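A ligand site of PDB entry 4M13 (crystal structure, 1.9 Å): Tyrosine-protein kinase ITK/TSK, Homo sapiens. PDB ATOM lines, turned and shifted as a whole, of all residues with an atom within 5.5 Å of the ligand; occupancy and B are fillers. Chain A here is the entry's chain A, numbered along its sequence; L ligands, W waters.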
ATOM      1  N   TRP A   5      33.093  -1.260  22.206  1.00  0.00           N
ATOM      2  CA  TRP A   5      32.073  -2.072  22.836  1.00  0.00           C
ATOM      3  C   TRP A   5      31.646  -3.280  21.967  1.00  0.00           C
ATOM      4  O   TRP A   5      30.979  -4.156  22.476  1.00  0.00           O
ATOM      5  CB  TRP A   5      30.871  -1.195  23.206  1.00  0.00           C
ATOM      6  CG  TRP A   5      30.503  -0.250  22.121  1.00  0.00           C
ATOM      7  CD1 TRP A   5      31.071   0.971  21.862  1.00  0.00           C
ATOM      8  CD2 TRP A   5      29.583  -0.495  21.060  1.00  0.00           C
ATOM      9  NE1 TRP A   5      30.530   1.506  20.729  1.00  0.00           N
ATOM     10  CE2 TRP A   5      29.625   0.628  20.207  1.00  0.00           C
ATOM     11  CE3 TRP A   5      28.693  -1.534  20.767  1.00  0.00           C
ATOM     12  CZ2 TRP A   5      28.801   0.750  19.090  1.00  0.00           C
ATOM     13  CZ3 TRP A   5      27.885  -1.426  19.655  1.00  0.00           C
ATOM     14  CH2 TRP A   5      27.967  -0.312  18.806  1.00  0.00           C
ATOM     15  N   PHE A  52      19.724   0.353  22.591  1.00  0.00           N
ATOM     16  CA  PHE A  52      20.787  -0.120  23.456  1.00  0.00           C
ATOM     17  C   PHE A  52      22.169   0.232  22.870  1.00  0.00           C
ATOM     18  O   PHE A  52      22.941   0.924  23.528  1.00  0.00           O
ATOM     19  CB  PHE A  52      20.647  -1.629  23.666  1.00  0.00           C
ATOM     20  CG  PHE A  52      21.731  -2.217  24.531  1.00  0.00           C
ATOM     21  CD1 PHE A  52      21.671  -2.084  25.918  1.00  0.00           C
ATOM     22  CD2 PHE A  52      22.814  -2.882  23.966  1.00  0.00           C
ATOM     23  CE1 PHE A  52      22.685  -2.619  26.723  1.00  0.00           C
ATOM     24  CE2 PHE A  52      23.829  -3.388  24.768  1.00  0.00           C
ATOM     25  CZ  PHE A  52      23.753  -3.264  26.141  1.00  0.00           C
ATOM     26  N   ILE A  53      22.441  -0.235  21.632  1.00  0.00           N
ATOM     27  CA  ILE A  53      23.700  -0.038  20.885  1.00  0.00           C
ATOM     28  C   ILE A  53      24.099   1.470  20.840  1.00  0.00           C
ATOM     29  O   ILE A  53      25.261   1.815  21.017  1.00  0.00           O
ATOM     30  CB  ILE A  53      23.563  -0.698  19.471  1.00  0.00           C
ATOM     31  CG1 ILE A  53      23.717  -2.232  19.576  1.00  0.00           C
ATOM     32  CG2 ILE A  53      24.508  -0.127  18.431  1.00  0.00           C
ATOM     33  CD1 ILE A  53      22.918  -3.063  18.474  1.00  0.00           C
ATOM     34  N   GLU A  55      23.558   3.855  22.975  1.00  0.00           N
ATOM     35  CA  GLU A  55      24.043   4.349  24.246  1.00  0.00           C
ATOM     36  C   GLU A  55      25.353   3.693  24.707  1.00  0.00           C
ATOM     37  O   GLU A  55      25.913   4.132  25.701  1.00  0.00           O
ATOM     38  CB  GLU A  55      22.971   4.160  25.337  1.00  0.00           C
ATOM     39  CG  GLU A  55      21.676   4.955  25.113  1.00  0.00           C
ATOM     40  CD  GLU A  55      20.649   4.859  26.229  1.00  0.00           C
ATOM     41  OE1 GLU A  55      21.027   4.605  27.394  1.00  0.00           O
ATOM     42  OE2 GLU A  55      19.456   5.123  25.946  1.00  0.00           O
ATOM     43  N   ALA A  56      25.804   2.635  24.002  1.00  0.00           N
ATOM     44  CA  ALA A  56      26.997   1.846  24.375  1.00  0.00           C
ATOM     45  C   ALA A  56      28.292   2.610  24.598  1.00  0.00           C
ATOM     46  O   ALA A  56      28.923   2.387  25.627  1.00  0.00           O
ATOM     47  CB  ALA A  56      27.213   0.673  23.427  1.00  0.00           C
ATOM     48  N   MET A  59      27.659   4.587  28.049  1.00  0.00           N
ATOM     49  CA  MET A  59      27.342   3.713  29.181  1.00  0.00           C
ATOM     50  C   MET A  59      28.417   2.670  29.522  1.00  0.00           C
ATOM     51  O   MET A  59      28.493   2.244  30.680  1.00  0.00           O
ATOM     52  CB  MET A  59      25.954   3.044  29.006  1.00  0.00           C
ATOM     53  CG  MET A  59      24.804   4.052  28.894  1.00  0.00           C
ATOM     54  SD  MET A  59      24.671   5.122  30.369  1.00  0.00           S
ATOM     55  CE  MET A  59      23.804   4.033  31.461  1.00  0.00           C
ATOM     56  N   MET A  60      29.232   2.256  28.541  1.00  0.00           N
ATOM     57  CA  MET A  60      30.296   1.277  28.814  1.00  0.00           C
ATOM     58  C   MET A  60      31.372   1.838  29.761  1.00  0.00           C
ATOM     59  O   MET A  60      32.078   1.065  30.412  1.00  0.00           O
ATOM     60  CB  MET A  60      30.936   0.743  27.505  1.00  0.00           C
ATOM     61  CG  MET A  60      31.921   1.712  26.867  1.00  0.00           C
ATOM     62  SD  MET A  60      32.658   1.091  25.318  1.00  0.00           S
ATOM     63  CE  MET A  60      33.870  -0.104  25.963  1.00  0.00           C
ATOM     64  N   LYS A  61      31.471   3.179  29.830  1.00  0.00           N
ATOM     65  CA  LYS A  61      32.440   3.882  30.671  1.00  0.00           C
ATOM     66  C   LYS A  61      32.132   3.746  32.168  1.00  0.00           C
ATOM     67  O   LYS A  61      33.046   3.957  32.978  1.00  0.00           O
ATOM     68  CB  LYS A  61      32.491   5.370  30.294  1.00  0.00           C
ATOM     69  CG  LYS A  61      33.120   5.642  28.931  1.00  0.00           C
ATOM     70  CD  LYS A  61      32.776   7.044  28.451  1.00  0.00           C
ATOM     71  CE  LYS A  61      33.652   7.536  27.317  1.00  0.00           C
ATOM     72  NZ  LYS A  61      33.472   6.740  26.071  1.00  0.00           N
ATOM     73  N   LEU A  62      30.858   3.452  32.541  1.00  0.00           N
ATOM     74  CA  LEU A  62      30.482   3.287  33.951  1.00  0.00           C
ATOM     75  C   LEU A  62      31.227   2.076  34.510  1.00  0.00           C
ATOM     76  O   LEU A  62      31.160   0.990  33.924  1.00  0.00           O
ATOM     77  CB  LEU A  62      28.967   3.091  34.142  1.00  0.00           C
ATOM     78  CG  LEU A  62      28.070   4.284  33.814  1.00  0.00           C
ATOM     79  CD1 LEU A  62      26.648   3.825  33.593  1.00  0.00           C
ATOM     80  CD2 LEU A  62      28.114   5.333  34.904  1.00  0.00           C
ATOM     81  N   SER A  63      31.959   2.282  35.598  1.00  0.00           N
ATOM     82  CA  SER A  63      32.778   1.222  36.197  1.00  0.00           C
ATOM     83  C   SER A  63      32.908   1.449  37.685  1.00  0.00           C
ATOM     84  O   SER A  63      33.227   2.570  38.113  1.00  0.00           O
ATOM     85  CB  SER A  63      34.164   1.198  35.564  1.00  0.00           C
ATOM     86  OG  SER A  63      34.966   0.202  36.166  1.00  0.00           O
ATOM     87  N   VAL A  68      28.526  -4.882  38.358  1.00  0.00           N
ATOM     88  CA  VAL A  68      28.954  -5.962  37.443  1.00  0.00           C
ATOM     89  C   VAL A  68      29.314  -5.266  36.140  1.00  0.00           C
ATOM     90  O   VAL A  68      28.463  -4.570  35.577  1.00  0.00           O
ATOM     91  CB  VAL A  68      27.834  -7.033  37.220  1.00  0.00           C
ATOM     92  CG1 VAL A  68      28.264  -8.085  36.169  1.00  0.00           C
ATOM     93  CG2 VAL A  68      27.432  -7.713  38.531  1.00  0.00           C
ATOM     94  N   GLN A  69      30.571  -5.424  35.658  1.00  0.00           N
ATOM     95  CA  GLN A  69      30.980  -4.781  34.403  1.00  0.00           C
ATOM     96  C   GLN A  69      30.339  -5.482  33.192  1.00  0.00           C
ATOM     97  O   GLN A  69      30.427  -6.702  33.078  1.00  0.00           O
ATOM     98  CB  GLN A  69      32.511  -4.772  34.265  1.00  0.00           C
ATOM     99  CG  GLN A  69      33.046  -3.840  33.168  1.00  0.00           C
ATOM    100  CD  GLN A  69      33.062  -2.388  33.568  1.00  0.00           C
ATOM    101  OE1 GLN A  69      33.661  -1.999  34.571  1.00  0.00           O
ATOM    102  NE2 GLN A  69      32.444  -1.537  32.756  1.00  0.00           N
ATOM    103  N   LEU A  70      29.741  -4.707  32.288  1.00  0.00           N
ATOM    104  CA  LEU A  70      29.189  -5.218  31.028  1.00  0.00           C
ATOM    105  C   LEU A  70      30.251  -4.743  30.007  1.00  0.00           C
ATOM    106  O   LEU A  70      30.353  -3.545  29.730  1.00  0.00           O
ATOM    107  CB  LEU A  70      27.786  -4.655  30.721  1.00  0.00           C
ATOM    108  CG  LEU A  70      27.189  -4.862  29.289  1.00  0.00           C
ATOM    109  CD1 LEU A  70      27.308  -6.310  28.790  1.00  0.00           C
ATOM    110  CD2 LEU A  70      25.713  -4.423  29.250  1.00  0.00           C
ATOM    111  N   TYR A  71      31.093  -5.678  29.537  1.00  0.00           N
ATOM    112  CA  TYR A  71      32.238  -5.409  28.683  1.00  0.00           C
ATOM    113  C   TYR A  71      31.932  -5.032  27.249  1.00  0.00           C
ATOM    114  O   TYR A  71      32.669  -4.264  26.626  1.00  0.00           O
ATOM    115  CB  TYR A  71      33.169  -6.620  28.673  1.00  0.00           C
ATOM    116  CG  TYR A  71      33.793  -6.937  30.004  1.00  0.00           C
ATOM    117  CD1 TYR A  71      34.612  -6.012  30.664  1.00  0.00           C
ATOM    118  CD2 TYR A  71      33.651  -8.200  30.572  1.00  0.00           C
ATOM    119  CE1 TYR A  71      35.221  -6.320  31.878  1.00  0.00           C
ATOM    120  CE2 TYR A  71      34.272  -8.524  31.782  1.00  0.00           C
ATOM    121  CZ  TYR A  71      35.038  -7.575  32.443  1.00  0.00           C
ATOM    122  OH  TYR A  71      35.684  -7.904  33.608  1.00  0.00           O
ATOM    123  N   GLY A  72      30.890  -5.635  26.713  1.00  0.00           N
ATOM    124  CA  GLY A  72      30.536  -5.377  25.336  1.00  0.00           C
ATOM    125  C   GLY A  72      29.455  -6.276  24.811  1.00  0.00           C
ATOM    126  O   GLY A  72      28.883  -7.080  25.558  1.00  0.00           O
ATOM    127  N   VAL A  73      29.172  -6.105  23.518  1.00  0.00           N
ATOM    128  CA  VAL A  73      28.103  -6.810  22.814  1.00  0.00           C
ATOM    129  C   VAL A  73      28.634  -7.492  21.537  1.00  0.00           C
ATOM    130  O   VAL A  73      29.418  -6.897  20.784  1.00  0.00           O
ATOM    131  CB  VAL A  73      26.885  -5.874  22.541  1.00  0.00           C
ATOM    132  CG1 VAL A  73      27.292  -4.616  21.767  1.00  0.00           C
ATOM    133  CG2 VAL A  73      25.728  -6.596  21.837  1.00  0.00           C
ATOM    134  N   LEU A  82      25.379 -10.460  25.249  1.00  0.00           N
ATOM    135  CA  LEU A  82      25.936  -9.447  26.151  1.00  0.00           C
ATOM    136  C   LEU A  82      27.050 -10.128  26.964  1.00  0.00           C
ATOM    137  O   LEU A  82      26.857 -11.257  27.434  1.00  0.00           O
ATOM    138  CB  LEU A  82      24.834  -8.859  27.054  1.00  0.00           C
ATOM    139  CG  LEU A  82      23.805  -7.963  26.359  1.00  0.00           C
ATOM    140  CD1 LEU A  82      22.783  -7.422  27.373  1.00  0.00           C
ATOM    141  CD2 LEU A  82      24.476  -6.808  25.667  1.00  0.00           C
ATOM    142  N   PHE A  84      29.576 -10.067  30.128  1.00  0.00           N
ATOM    143  CA  PHE A  84      29.746  -9.516  31.468  1.00  0.00           C
ATOM    144  C   PHE A  84      30.927 -10.122  32.210  1.00  0.00           C
ATOM    145  O   PHE A  84      31.396 -11.222  31.913  1.00  0.00           O
ATOM    146  CB  PHE A  84      28.482  -9.829  32.328  1.00  0.00           C
ATOM    147  CG  PHE A  84      27.171  -9.255  31.831  1.00  0.00           C
ATOM    148  CD1 PHE A  84      26.704  -8.036  32.306  1.00  0.00           C
ATOM    149  CD2 PHE A  84      26.400  -9.942  30.892  1.00  0.00           C
ATOM    150  CE1 PHE A  84      25.464  -7.535  31.892  1.00  0.00           C
ATOM    151  CE2 PHE A  84      25.163  -9.435  30.465  1.00  0.00           C
ATOM    152  CZ  PHE A  84      24.689  -8.233  30.979  1.00  0.00           C
ATOM    153  N   VAL A 147      25.807  -4.746  41.774  1.00  0.00           N
ATOM    154  CA  VAL A 147      24.525  -4.445  41.130  1.00  0.00           C
ATOM    155  C   VAL A 147      24.674  -4.680  39.620  1.00  0.00           C
ATOM    156  O   VAL A 147      25.730  -4.406  39.042  1.00  0.00           O
ATOM    157  CB  VAL A 147      24.103  -2.989  41.452  1.00  0.00           C
ATOM    158  CG1 VAL A 147      22.796  -2.628  40.759  1.00  0.00           C
ATOM    159  CG2 VAL A 147      23.995  -2.748  42.964  1.00  0.00           C
ATOM    160  N   SER A 148      23.618  -5.195  38.971  1.00  0.00           N
ATOM    161  CA  SER A 148      23.636  -5.437  37.535  1.00  0.00           C
ATOM    162  C   SER A 148      22.298  -5.060  36.923  1.00  0.00           C
ATOM    163  O   SER A 148      21.333  -4.851  37.660  1.00  0.00           O
ATOM    164  CB  SER A 148      23.929  -6.923  37.279  1.00  0.00           C
ATOM    165  OG  SER A 148      24.196  -7.156  35.901  1.00  0.00           O
ATOM    166  N   ASP A 149      22.240  -4.932  35.581  1.00  0.00           N
ATOM    167  CA  ASP A 149      21.028  -4.693  34.798  1.00  0.00           C
ATOM    168  C   ASP A 149      20.392  -3.320  35.052  1.00  0.00           C
ATOM    169  O   ASP A 149      19.194  -3.127  34.822  1.00  0.00           O
ATOM    170  CB  ASP A 149      20.007  -5.850  35.001  1.00  0.00           C
ATOM    171  CG  ASP A 149      20.480  -7.264  34.629  1.00  0.00           C
ATOM    172  OD1 ASP A 149      21.578  -7.404  34.056  1.00  0.00           O
ATOM    173  OD2 ASP A 149      19.742  -8.224  34.924  1.00  0.00           O
ATOM    174  N   PHE A 150      21.191  -2.356  35.529  1.00  0.00           N
ATOM    175  CA  PHE A 150      20.700  -0.992  35.758  1.00  0.00           C
ATOM    176  C   PHE A 150      20.336  -0.388  34.422  1.00  0.00           C
ATOM    177  O   PHE A 150      21.065  -0.578  33.430  1.00  0.00           O
ATOM    178  CB  PHE A 150      21.721  -0.122  36.526  1.00  0.00           C
ATOM    179  CG  PHE A 150      23.179  -0.336  36.198  1.00  0.00           C
ATOM    180  CD1 PHE A 150      23.798   0.410  35.199  1.00  0.00           C
ATOM    181  CD2 PHE A 150      23.921  -1.285  36.880  1.00  0.00           C
ATOM    182  CE1 PHE A 150      25.152   0.210  34.897  1.00  0.00           C
ATOM    183  CE2 PHE A 150      25.283  -1.461  36.606  1.00  0.00           C
ATOM    184  CZ  PHE A 150      25.889  -0.713  35.613  1.00  0.00           C
ATOM    185  N   GLY A 151      19.172   0.253  34.404  1.00  0.00           N
ATOM    186  CA  GLY A 151      18.606   0.934  33.237  1.00  0.00           C
ATOM    187  C   GLY A 151      18.048   0.048  32.125  1.00  0.00           C
ATOM    188  O   GLY A 151      17.432   0.557  31.186  1.00  0.00           O
ATOM    189  N   MET A 152      18.217  -1.279  32.237  1.00  0.00           N
ATOM    190  CA  MET A 152      17.823  -2.237  31.185  1.00  0.00           C
ATOM    191  C   MET A 152      16.323  -2.301  30.834  1.00  0.00           C
ATOM    192  O   MET A 152      15.995  -2.631  29.696  1.00  0.00           O
ATOM    193  CB  MET A 152      18.416  -3.638  31.444  1.00  0.00           C
ATOM    194  CG  MET A 152      19.943  -3.648  31.454  1.00  0.00           C
ATOM    195  SD  MET A 152      20.798  -3.052  29.954  1.00  0.00           S
ATOM    196  CE  MET A 152      20.300  -4.351  28.804  1.00  0.00           C
ATOM    197  N   ARG A 154      14.507   0.086  30.166  1.00  0.00           N
ATOM    198  CA  ARG A 154      14.261   1.101  29.126  1.00  0.00           C
ATOM    199  C   ARG A 154      14.309   0.464  27.733  1.00  0.00           C
ATOM    200  O   ARG A 154      13.816   1.050  26.773  1.00  0.00           O
ATOM    201  CB  ARG A 154      15.316   2.230  29.199  1.00  0.00           C
ATOM    202  CG  ARG A 154      15.170   3.130  30.416  1.00  0.00           C
ATOM    203  CD  ARG A 154      16.003   4.394  30.327  1.00  0.00           C
ATOM    204  NE  ARG A 154      17.448   4.153  30.408  1.00  0.00           N
ATOM    205  CZ  ARG A 154      18.295   4.224  29.380  1.00  0.00           C
ATOM    206  NH1 ARG A 154      17.833   4.468  28.157  1.00  0.00           N
ATOM    207  NH2 ARG A 154      19.590   4.058  29.561  1.00  0.00           N
ATOM    208  N   PHE A 155      14.889  -0.735  27.625  1.00  0.00           N
ATOM    209  CA  PHE A 155      15.023  -1.461  26.365  1.00  0.00           C
ATOM    210  C   PHE A 155      14.104  -2.679  26.247  1.00  0.00           C
ATOM    211  O   PHE A 155      13.955  -3.186  25.126  1.00  0.00           O
ATOM    212  CB  PHE A 155      16.489  -1.866  26.127  1.00  0.00           C
ATOM    213  CG  PHE A 155      17.411  -0.707  26.361  1.00  0.00           C
ATOM    214  CD1 PHE A 155      17.471   0.353  25.460  1.00  0.00           C
ATOM    215  CD2 PHE A 155      18.192  -0.638  27.515  1.00  0.00           C
ATOM    216  CE1 PHE A 155      18.306   1.453  25.707  1.00  0.00           C
ATOM    217  CE2 PHE A 155      19.030   0.454  27.751  1.00  0.00           C
ATOM    218  CZ  PHE A 155      19.074   1.492  26.837  1.00  0.00           C
HETATM  219  N1  LIG L   1      24.983  -0.770  31.378  1.00  0.00           N
HETATM  220  N2  LIG L   1      26.264  -0.356  31.459  1.00  0.00           N
HETATM  221  C1  LIG L   1      26.888  -1.287  32.252  1.00  0.00           C
HETATM  222  C2  LIG L   1      25.950  -2.288  32.681  1.00  0.00           C
HETATM  223  C3  LIG L   1      24.716  -1.932  32.109  1.00  0.00           C
HETATM  224  N3  LIG L   1      26.283  -3.344  33.514  1.00  0.00           N
HETATM  225  C4  LIG L   1      25.340  -4.313  33.909  1.00  0.00           C
HETATM  226  N4  LIG L   1      25.827  -5.312  34.741  1.00  0.00           N
HETATM  227  O1  LIG L   1      24.160  -4.292  33.552  1.00  0.00           O
HETATM  228  C5  LIG L   1      28.309  -1.228  32.586  1.00  0.00           C
HETATM  229  N5  LIG L   1      29.035  -0.138  32.174  1.00  0.00           N
HETATM  230  O2  LIG L   1      28.854  -2.151  33.228  1.00  0.00           O
HETATM  231  C6  LIG L   1      24.017  -0.090  30.560  1.00  0.00           C
HETATM  232  C7  LIG L   1      22.916   0.454  31.177  1.00  0.00           C
HETATM  233  C8  LIG L   1      21.956   1.130  30.390  1.00  0.00           C
HETATM  234  C9  LIG L   1      22.128   1.260  29.037  1.00  0.00           C
HETATM  235  C10 LIG L   1      24.232   0.012  29.155  1.00  0.00           C
HETATM  236  C11 LIG L   1      23.260   0.693  28.407  1.00  0.00           C
HETATM  237  C12 LIG L   1      23.431   0.801  26.989  1.00  0.00           C
HETATM  238  C13 LIG L   1      24.513   0.267  26.380  1.00  0.00           C
HETATM  239  C14 LIG L   1      25.509  -0.405  27.161  1.00  0.00           C
HETATM  240  C15 LIG L   1      25.367  -0.536  28.511  1.00  0.00           C
HETATM  241  O3  LIG L   1      26.540  -0.874  26.415  1.00  0.00           O
HETATM  242  C16 LIG L   1      27.593  -1.528  27.111  1.00  0.00           C
HETATM  243  C17 LIG L   1      28.528  -2.065  26.027  1.00  0.00           C
HETATM  244  C18 LIG L   1      27.838  -3.142  25.206  1.00  0.00           C
HETATM  245  O   HOH W   1      30.265  -1.359  35.396  1.00  0.00           O
HETATM  246  O   HOH W   2      22.553  -5.615  31.458  1.00  0.00           O
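Water W1 lies within hydrogen-bond range of O2 of the ligand, O of Leu 62 and NE2 of Gln 69.
Residues that only touch the ligand: Trp 5 (3.8 Å), Phe 52 (3.3 Å), Glu 55 (3.8 Å), Ala 56 (3.4 Å), Met 60 (3.7 Å), Gln 69 (3.6 Å), Gly 72 (3.5 Å), Val 73 (3.7 Å), Phe 84 (3.6 Å), Phe 150 (3.1 Å), Arg 154 (3.8 Å) and Phe 155 (3.4 Å). Hydrophobic or aromatic side chains within 4 Å of the ligand: Trp 5, Phe 52, Ala 56, Met 59, Met 60, Leu 62, Val 68, Leu 70, Val 73, Phe 84, Phe 150 and Phe 155. The nearest printed residue that does not touch the ligand is Met 152 (4.3 Å).
The side-chain hydroxyl (OG) of Ser 148 lies within hydrogen-bond range of the side-chain carboxylate (OD1) of Asp 149. The backbone NH (N) of Val 68 is in hydrogen-bond range of the backbone carbonyl oxygen (O) of Val 147, 2.9 Å away. The backbone carbonyl oxygen (O) of Leu 62 lies within hydrogen-bond range of the side-chain amide nitrogen (NE2) of Gln 69 (3.1 Å). OE1 of Gln 69 lies within hydrogen-bond range of OG of Ser 63. N of Val 73 sits at hydrogen-bond distance from O of Trp 5 (2.9 Å). OE1 of Glu 55 lies within salt-bridge range of NH2 of Arg 154, 2.7 Å away.
OG of Ser 148 lies within hydrogen-bond range of N4 of the ligand (2.7 Å). A nitrogen (N4) of the ligand is in hydrogen-bond range of the backbone carbonyl oxygen of Val 68, 2.9 Å away. The backbone carbonyl oxygen of Met 59 lies within hydrogen-bond range of a nitrogen (N5) of the ligand (2.9 Å). An oxygen (O2) of the ligand sits at hydrogen-bond distance from the backbone NH of Leu 70, at 2.9 Å. N of Asp 149 is in hydrogen-bond range of O1 of the ligand. The backbone carbonyl oxygen (O) of Leu 62 lies within hydrogen-bond range of a nitrogen (N5) of the ligand.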
